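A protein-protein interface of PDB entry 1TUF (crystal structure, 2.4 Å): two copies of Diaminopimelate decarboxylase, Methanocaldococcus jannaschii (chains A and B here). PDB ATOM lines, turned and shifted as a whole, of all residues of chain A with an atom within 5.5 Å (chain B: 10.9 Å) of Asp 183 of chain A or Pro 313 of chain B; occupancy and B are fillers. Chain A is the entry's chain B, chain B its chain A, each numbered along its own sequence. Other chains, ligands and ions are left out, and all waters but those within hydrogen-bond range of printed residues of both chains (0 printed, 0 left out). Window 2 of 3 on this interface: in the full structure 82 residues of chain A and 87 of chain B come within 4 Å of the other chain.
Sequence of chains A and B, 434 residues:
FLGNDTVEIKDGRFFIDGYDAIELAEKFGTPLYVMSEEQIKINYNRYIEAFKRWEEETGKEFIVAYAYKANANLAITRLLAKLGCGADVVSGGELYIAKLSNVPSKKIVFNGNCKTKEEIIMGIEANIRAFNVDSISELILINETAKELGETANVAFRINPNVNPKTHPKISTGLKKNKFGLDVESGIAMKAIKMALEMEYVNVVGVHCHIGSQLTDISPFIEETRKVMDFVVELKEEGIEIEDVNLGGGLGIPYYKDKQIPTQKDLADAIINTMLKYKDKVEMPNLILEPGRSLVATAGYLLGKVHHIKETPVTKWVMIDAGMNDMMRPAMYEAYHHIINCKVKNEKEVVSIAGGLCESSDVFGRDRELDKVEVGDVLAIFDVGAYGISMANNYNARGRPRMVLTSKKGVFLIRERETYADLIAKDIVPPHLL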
ATOM      1  N   ASN A 160      19.390 -21.940   5.047  1.00  0.00           N
ATOM      2  CA  ASN A 160      18.160 -21.255   4.688  1.00  0.00           C
ATOM      3  C   ASN A 160      18.326 -20.829   3.237  1.00  0.00           C
ATOM      4  O   ASN A 160      19.046 -19.881   2.933  1.00  0.00           O
ATOM      5  CB  ASN A 160      17.911 -20.023   5.565  1.00  0.00           C
ATOM      6  CG  ASN A 160      18.044 -20.315   7.049  1.00  0.00           C
ATOM      7  OD1 ASN A 160      17.627 -21.369   7.540  1.00  0.00           O
ATOM      8  ND2 ASN A 160      18.622 -19.363   7.777  1.00  0.00           N
ATOM      9  N   LEU A 175      12.719 -17.658   6.370  1.00  0.00           N
ATOM     10  CA  LEU A 175      14.123 -18.021   6.203  1.00  0.00           C
ATOM     11  C   LEU A 175      15.050 -16.804   6.185  1.00  0.00           C
ATOM     12  O   LEU A 175      16.233 -16.928   5.871  1.00  0.00           O
ATOM     13  CB  LEU A 175      14.312 -18.833   4.914  1.00  0.00           C
ATOM     14  CG  LEU A 175      13.687 -20.234   4.845  1.00  0.00           C
ATOM     15  CD1 LEU A 175      13.831 -20.788   3.436  1.00  0.00           C
ATOM     16  CD2 LEU A 175      14.363 -21.158   5.853  1.00  0.00           C
ATOM     17  N   LYS A 176      14.519 -15.632   6.523  1.00  0.00           N
ATOM     18  CA  LYS A 176      15.323 -14.412   6.533  1.00  0.00           C
ATOM     19  C   LYS A 176      15.246 -13.644   7.846  1.00  0.00           C
ATOM     20  O   LYS A 176      16.255 -13.133   8.333  1.00  0.00           O
ATOM     21  CB  LYS A 176      14.902 -13.489   5.386  1.00  0.00           C
ATOM     22  CG  LYS A 176      15.437 -13.894   4.023  1.00  0.00           C
ATOM     23  CD  LYS A 176      14.944 -12.945   2.937  1.00  0.00           C
ATOM     24  CE  LYS A 176      15.556 -13.270   1.572  1.00  0.00           C
ATOM     25  NZ  LYS A 176      17.037 -13.063   1.530  1.00  0.00           N
ATOM     26  N   GLY A 181      18.823 -21.594  11.183  1.00  0.00           N
ATOM     27  CA  GLY A 181      19.706 -21.801  10.052  1.00  0.00           C
ATOM     28  C   GLY A 181      20.828 -20.852   9.707  1.00  0.00           C
ATOM     29  O   GLY A 181      21.013 -19.795  10.315  1.00  0.00           O
ATOM     30  N   LEU A 182      21.581 -21.262   8.692  1.00  0.00           N
ATOM     31  CA  LEU A 182      22.711 -20.497   8.187  1.00  0.00           C
ATOM     32  C   LEU A 182      22.319 -19.961   6.810  1.00  0.00           C
ATOM     33  O   LEU A 182      21.989 -20.726   5.905  1.00  0.00           O
ATOM     34  CB  LEU A 182      23.934 -21.409   8.092  1.00  0.00           C
ATOM     35  CG  LEU A 182      24.351 -22.097   9.402  1.00  0.00           C
ATOM     36  CD1 LEU A 182      25.049 -23.414   9.096  1.00  0.00           C
ATOM     37  CD2 LEU A 182      25.263 -21.172  10.202  1.00  0.00           C
ATOM     38  N   ASP A 183      22.332 -18.641   6.669  1.00  0.00           N
ATOM     39  CA  ASP A 183      21.961 -17.997   5.415  1.00  0.00           C
ATOM     40  C   ASP A 183      22.822 -18.511   4.258  1.00  0.00           C
ATOM     41  O   ASP A 183      24.045 -18.641   4.376  1.00  0.00           O
ATOM     42  CB  ASP A 183      22.099 -16.471   5.555  1.00  0.00           C
ATOM     43  CG  ASP A 183      21.408 -15.707   4.434  1.00  0.00           C
ATOM     44  OD1 ASP A 183      22.090 -14.939   3.735  1.00  0.00           O
ATOM     45  OD2 ASP A 183      20.183 -15.864   4.254  1.00  0.00           O
ATOM     46  N   VAL A 184      22.181 -18.822   3.142  1.00  0.00           N
ATOM     47  CA  VAL A 184      22.911 -19.317   1.995  1.00  0.00           C
ATOM     48  C   VAL A 184      23.385 -18.135   1.159  1.00  0.00           C
ATOM     49  O   VAL A 184      24.577 -17.999   0.889  1.00  0.00           O
ATOM     50  CB  VAL A 184      22.026 -20.256   1.139  1.00  0.00           C
ATOM     51  CG1 VAL A 184      22.674 -20.514  -0.204  1.00  0.00           C
ATOM     52  CG2 VAL A 184      21.804 -21.569   1.879  1.00  0.00           C
ATOM     53  N   GLU A 185      22.445 -17.272   0.782  1.00  0.00           N
ATOM     54  CA  GLU A 185      22.732 -16.096  -0.028  1.00  0.00           C
ATOM     55  C   GLU A 185      23.965 -15.312   0.396  1.00  0.00           C
ATOM     56  O   GLU A 185      24.844 -15.042  -0.419  1.00  0.00           O
ATOM     57  CB  GLU A 185      21.523 -15.156  -0.029  1.00  0.00           C
ATOM     58  CG  GLU A 185      21.777 -13.797  -0.672  1.00  0.00           C
ATOM     59  CD  GLU A 185      20.501 -12.975  -0.830  1.00  0.00           C
ATOM     60  OE1 GLU A 185      19.725 -12.892   0.149  1.00  0.00           O
ATOM     61  OE2 GLU A 185      20.277 -12.412  -1.929  1.00  0.00           O
ATOM     62  N   SER A 186      24.021 -14.950   1.672  1.00  0.00           N
ATOM     63  CA  SER A 186      25.126 -14.163   2.200  1.00  0.00           C
ATOM     64  C   SER A 186      26.450 -14.921   2.277  1.00  0.00           C
ATOM     65  O   SER A 186      27.480 -14.337   2.621  1.00  0.00           O
ATOM     66  CB  SER A 186      24.762 -13.623   3.588  1.00  0.00           C
ATOM     67  OG  SER A 186      24.470 -14.684   4.476  1.00  0.00           O
ATOM     68  N   GLY A 187      26.420 -16.214   1.973  1.00  0.00           N
ATOM     69  CA  GLY A 187      27.633 -17.013   2.013  1.00  0.00           C
ATOM     70  C   GLY A 187      27.942 -17.636   3.360  1.00  0.00           C
ATOM     71  O   GLY A 187      28.927 -18.368   3.503  1.00  0.00           O
ATOM     72  N   ILE A 188      27.096 -17.358   4.347  1.00  0.00           N
ATOM     73  CA  ILE A 188      27.293 -17.885   5.689  1.00  0.00           C
ATOM     74  C   ILE A 188      27.294 -19.414   5.737  1.00  0.00           C
ATOM     75  O   ILE A 188      28.122 -20.019   6.418  1.00  0.00           O
ATOM     76  CB  ILE A 188      26.219 -17.334   6.657  1.00  0.00           C
ATOM     77  CG1 ILE A 188      26.388 -15.811   6.791  1.00  0.00           C
ATOM     78  CG2 ILE A 188      26.329 -18.024   8.013  1.00  0.00           C
ATOM     79  CD1 ILE A 188      25.391 -15.138   7.736  1.00  0.00           C
ATOM     80  N   ALA A 189      26.374 -20.043   5.016  1.00  0.00           N
ATOM     81  CA  ALA A 189      26.304 -21.495   5.012  1.00  0.00           C
ATOM     82  C   ALA A 189      27.615 -22.089   4.520  1.00  0.00           C
ATOM     83  O   ALA A 189      28.189 -22.972   5.162  1.00  0.00           O
ATOM     84  CB  ALA A 189      25.151 -21.961   4.132  1.00  0.00           C
ATOM     85  N   MET A 190      28.083 -21.597   3.379  1.00  0.00           N
ATOM     86  CA  MET A 190      29.331 -22.067   2.793  1.00  0.00           C
ATOM     87  C   MET A 190      30.468 -21.869   3.796  1.00  0.00           C
ATOM     88  O   MET A 190      31.259 -22.782   4.053  1.00  0.00           O
ATOM     89  CB  MET A 190      29.617 -21.284   1.509  1.00  0.00           C
ATOM     90  CG  MET A 190      30.831 -21.750   0.725  1.00  0.00           C
ATOM     91  SD  MET A 190      30.571 -23.348  -0.086  1.00  0.00           S
ATOM     92  CE  MET A 190      31.627 -24.321   0.887  1.00  0.00           C
ATOM     93  N   LYS B 310      24.514 -15.288  17.533  1.00  0.00           N
ATOM     94  CA  LYS B 310      24.470 -15.587  16.113  1.00  0.00           C
ATOM     95  C   LYS B 310      24.227 -14.321  15.320  1.00  0.00           C
ATOM     96  O   LYS B 310      23.231 -13.626  15.521  1.00  0.00           O
ATOM     97  CB  LYS B 310      23.355 -16.594  15.829  1.00  0.00           C
ATOM     98  CG  LYS B 310      23.161 -16.968  14.376  1.00  0.00           C
ATOM     99  CD  LYS B 310      21.885 -17.786  14.271  1.00  0.00           C
ATOM    100  CE  LYS B 310      21.730 -18.512  12.949  1.00  0.00           C
ATOM    101  NZ  LYS B 310      20.392 -19.157  12.922  1.00  0.00           N
ATOM    102  N   GLU B 311      25.142 -14.026  14.411  1.00  0.00           N
ATOM    103  CA  GLU B 311      25.013 -12.843  13.588  1.00  0.00           C
ATOM    104  C   GLU B 311      24.468 -13.206  12.208  1.00  0.00           C
ATOM    105  O   GLU B 311      24.954 -14.128  11.555  1.00  0.00           O
ATOM    106  CB  GLU B 311      26.374 -12.164  13.459  1.00  0.00           C
ATOM    107  CG  GLU B 311      26.275 -10.670  13.328  1.00  0.00           C
ATOM    108  CD  GLU B 311      27.596  -9.977  13.559  1.00  0.00           C
ATOM    109  OE1 GLU B 311      28.349 -10.428  14.448  1.00  0.00           O
ATOM    110  OE2 GLU B 311      27.872  -8.975  12.862  1.00  0.00           O
ATOM    111  N   THR B 312      23.440 -12.489  11.774  1.00  0.00           N
ATOM    112  CA  THR B 312      22.856 -12.731  10.466  1.00  0.00           C
ATOM    113  C   THR B 312      22.931 -11.414   9.704  1.00  0.00           C
ATOM    114  O   THR B 312      23.142 -10.354  10.297  1.00  0.00           O
ATOM    115  CB  THR B 312      21.377 -13.181  10.568  1.00  0.00           C
ATOM    116  OG1 THR B 312      20.543 -12.053  10.858  1.00  0.00           O
ATOM    117  CG2 THR B 312      21.219 -14.222  11.659  1.00  0.00           C
ATOM    118  N   PRO B 313      22.758 -11.458   8.377  1.00  0.00           N
ATOM    119  CA  PRO B 313      22.817 -10.246   7.557  1.00  0.00           C
ATOM    120  C   PRO B 313      21.783  -9.165   7.891  1.00  0.00           C
ATOM    121  O   PRO B 313      21.923  -8.013   7.475  1.00  0.00           O
ATOM    122  CB  PRO B 313      22.661 -10.789   6.137  1.00  0.00           C
ATOM    123  CG  PRO B 313      21.832 -12.024   6.331  1.00  0.00           C
ATOM    124  CD  PRO B 313      22.476 -12.642   7.544  1.00  0.00           C
ATOM    125  N   VAL B 314      20.754  -9.520   8.649  1.00  0.00           N
ATOM    126  CA  VAL B 314      19.727  -8.542   8.987  1.00  0.00           C
ATOM    127  C   VAL B 314      19.467  -8.426  10.489  1.00  0.00           C
ATOM    128  O   VAL B 314      18.848  -7.464  10.941  1.00  0.00           O
ATOM    129  CB  VAL B 314      18.396  -8.888   8.284  1.00  0.00           C
ATOM    130  CG1 VAL B 314      17.835 -10.181   8.849  1.00  0.00           C
ATOM    131  CG2 VAL B 314      17.404  -7.751   8.456  1.00  0.00           C
ATOM    132  N   THR B 315      19.946  -9.396  11.260  1.00  0.00           N
ATOM    133  CA  THR B 315      19.722  -9.381  12.699  1.00  0.00           C
ATOM    134  C   THR B 315      20.855 -10.007  13.494  1.00  0.00           C
ATOM    135  O   THR B 315      21.560 -10.888  13.006  1.00  0.00           O
ATOM    136  CB  THR B 315      18.437 -10.146  13.059  1.00  0.00           C
ATOM    137  OG1 THR B 315      17.316  -9.537  12.409  1.00  0.00           O
ATOM    138  CG2 THR B 315      18.213 -10.139  14.557  1.00  0.00           C
ATOM    139  N   LYS B 316      21.033  -9.537  14.723  1.00  0.00           N
ATOM    140  CA  LYS B 316      22.045 -10.098  15.600  1.00  0.00           C
ATOM    141  C   LYS B 316      21.289 -10.842  16.694  1.00  0.00           C
ATOM    142  O   LYS B 316      20.683 -10.223  17.557  1.00  0.00           O
ATOM    143  CB  LYS B 316      22.903  -9.002  16.218  1.00  0.00           C
ATOM    144  CG  LYS B 316      24.079  -9.548  17.001  1.00  0.00           C
ATOM    145  CD  LYS B 316      25.124  -8.482  17.178  1.00  0.00           C
ATOM    146  CE  LYS B 316      26.494  -9.084  17.439  1.00  0.00           C
ATOM    147  NZ  LYS B 316      27.561  -8.036  17.415  1.00  0.00           N
ATOM    148  N   TRP B 317      21.329 -12.168  16.650  1.00  0.00           N
ATOM    149  CA  TRP B 317      20.614 -12.988  17.614  1.00  0.00           C
ATOM    150  C   TRP B 317      21.361 -13.385  18.885  1.00  0.00           C
ATOM    151  O   TRP B 317      22.513 -13.821  18.858  1.00  0.00           O
ATOM    152  CB  TRP B 317      20.095 -14.261  16.939  1.00  0.00           C
ATOM    153  CG  TRP B 317      19.010 -14.033  15.936  1.00  0.00           C
ATOM    154  CD1 TRP B 317      19.153 -13.928  14.584  1.00  0.00           C
ATOM    155  CD2 TRP B 317      17.610 -13.887  16.204  1.00  0.00           C
ATOM    156  NE1 TRP B 317      17.928 -13.728  13.990  1.00  0.00           N
ATOM    157  CE2 TRP B 317      16.963 -13.697  14.960  1.00  0.00           C
ATOM    158  CE3 TRP B 317      16.839 -13.897  17.374  1.00  0.00           C
ATOM    159  CZ2 TRP B 317      15.575 -13.521  14.852  1.00  0.00           C
ATOM    160  CZ3 TRP B 317      15.459 -13.722  17.270  1.00  0.00           C
ATOM    161  CH2 TRP B 317      14.842 -13.534  16.012  1.00  0.00           C
ATOM    162  N   VAL B 350      21.915  -3.141  19.329  1.00  0.00           N
ATOM    163  CA  VAL B 350      20.580  -3.624  19.032  1.00  0.00           C
ATOM    164  C   VAL B 350      20.611  -5.079  18.607  1.00  0.00           C
ATOM    165  O   VAL B 350      21.287  -5.450  17.649  1.00  0.00           O
ATOM    166  CB  VAL B 350      19.927  -2.795  17.935  1.00  0.00           C
ATOM    167  CG1 VAL B 350      18.512  -3.301  17.677  1.00  0.00           C
ATOM    168  CG2 VAL B 350      19.903  -1.343  18.351  1.00  0.00           C
ATOM    169  N   SER B 352      18.323  -9.194  18.950  1.00  0.00           N
ATOM    170  CA  SER B 352      17.074  -9.911  19.145  1.00  0.00           C
ATOM    171  C   SER B 352      17.341 -11.076  20.084  1.00  0.00           C
ATOM    172  O   SER B 352      18.326 -11.804  19.923  1.00  0.00           O
ATOM    173  CB  SER B 352      16.523 -10.411  17.810  1.00  0.00           C
ATOM    174  OG  SER B 352      15.977  -9.340  17.060  1.00  0.00           O
ATOM    175  N   ASP B 367      14.856  -6.297  17.968  1.00  0.00           N
ATOM    176  CA  ASP B 367      15.463  -4.980  17.834  1.00  0.00           C
ATOM    177  C   ASP B 367      15.546  -4.236  19.154  1.00  0.00           C
ATOM    178  O   ASP B 367      15.299  -3.036  19.217  1.00  0.00           O
ATOM    179  CB  ASP B 367      14.670  -4.142  16.823  1.00  0.00           C
ATOM    180  CG  ASP B 367      14.565  -4.813  15.467  1.00  0.00           C
ATOM    181  OD1 ASP B 367      15.617  -5.215  14.921  1.00  0.00           O
ATOM    182  OD2 ASP B 367      13.434  -4.936  14.945  1.00  0.00           O
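Lys 176 of chain A touches Val 314 of chain B.
CG of Pro 313 of chain B touches OD1 of Asp 183 of chain A, 3.9 Å away.
Glu 311 of chain B touches Ile 188 of chain A.
CD of Pro 313 of chain B touches CD1 of Ile 188 of chain A, 3.8 Å away.
Of the 13 printed residues of chain A, 4 touch a printed residue of chain B.
Printed residues of chain A that touch a printed residue of chain B: Lys 176, Gly 181, Asp 183 and Ile 188.
Hydrophobic or aromatic side chains of chain A that line the printed part of chain B: Ile 188.
Of the 11 printed residues of chain B, 4 touch a printed residue of chain A.
Among the printed residues, 5 pairs touch across the chains.
Among the printed residues, no Asp or Glu carboxylate lies within 4 Å of a Lys or Arg side-chain nitrogen of the other chain.
No position is printed for both chains.
No residue of chain B comes within 4 Å of Asn 160 of chain A.
Lys 176 of chain A touches just one residue of chain B: Val 314.
Gly 181 of chain A touches just one residue of chain B: Lys 310.
No residue of chain B comes within 4 Å of Leu 182 of chain A.
No residue of chain B comes within 4 Å of Val 184 of chain A.
Glu 185 of chain A touches none of the printed residues of chain B.
Gly 187 of chain A touches none of the printed residues of chain B.
Ile 188 of chain A touches just these residues of chain B: Glu 311 (3.97 Å) and Pro 313 (3.8 Å).
Met 190 of chain A touches none of the printed residues of chain B.
Printed residues of chain A within 4 Å of Lys 310 of chain B: Gly 181 (2.8 Å).
Of the printed residues of chain A, Glu 311 of chain B touches Ile 188 (3.97 Å).
Printed residues of chain A within 4 Å of Val 314 of chain B: Lys 176.
The nearest residue of chain A that does not touch Pro 313 of chain B is Ser 186 of chain A (4.2 Å).
The nearest printed residue of chain A that does not touch Val 314 of chain B is Ile 188 of chain A (7.3 Å).
The backbone carbonyl oxygen (O) of Lys 310 of chain B is in hydrogen-bond range of the backbone NH (N) of Trp 317 of chain B (2.6 Å).
N of Ile 188 of chain A sits at hydrogen-bond distance from O of Asp 183 of chain A (3.3 Å).
The side-chain amino group of Lys 316 of chain B lies within salt-bridge range of the side-chain carboxylate of Glu 311 of chain B (3.9 Å).
N of Ala 189 of chain A sits at hydrogen-bond distance from O of Asp 183 of chain A.
OG of Ser 186 of chain A is in hydrogen-bond range of OD1 of Asp 183 of chain A.
The side-chain hydroxyl of Thr 312 of chain B lies close to the backbone NH of Val 314 of chain B, 3.4 Å away.
NZ of Lys 310 of chain B lies within hydrogen-bond range of O of Gly 181 of chain A (2.8 Å).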
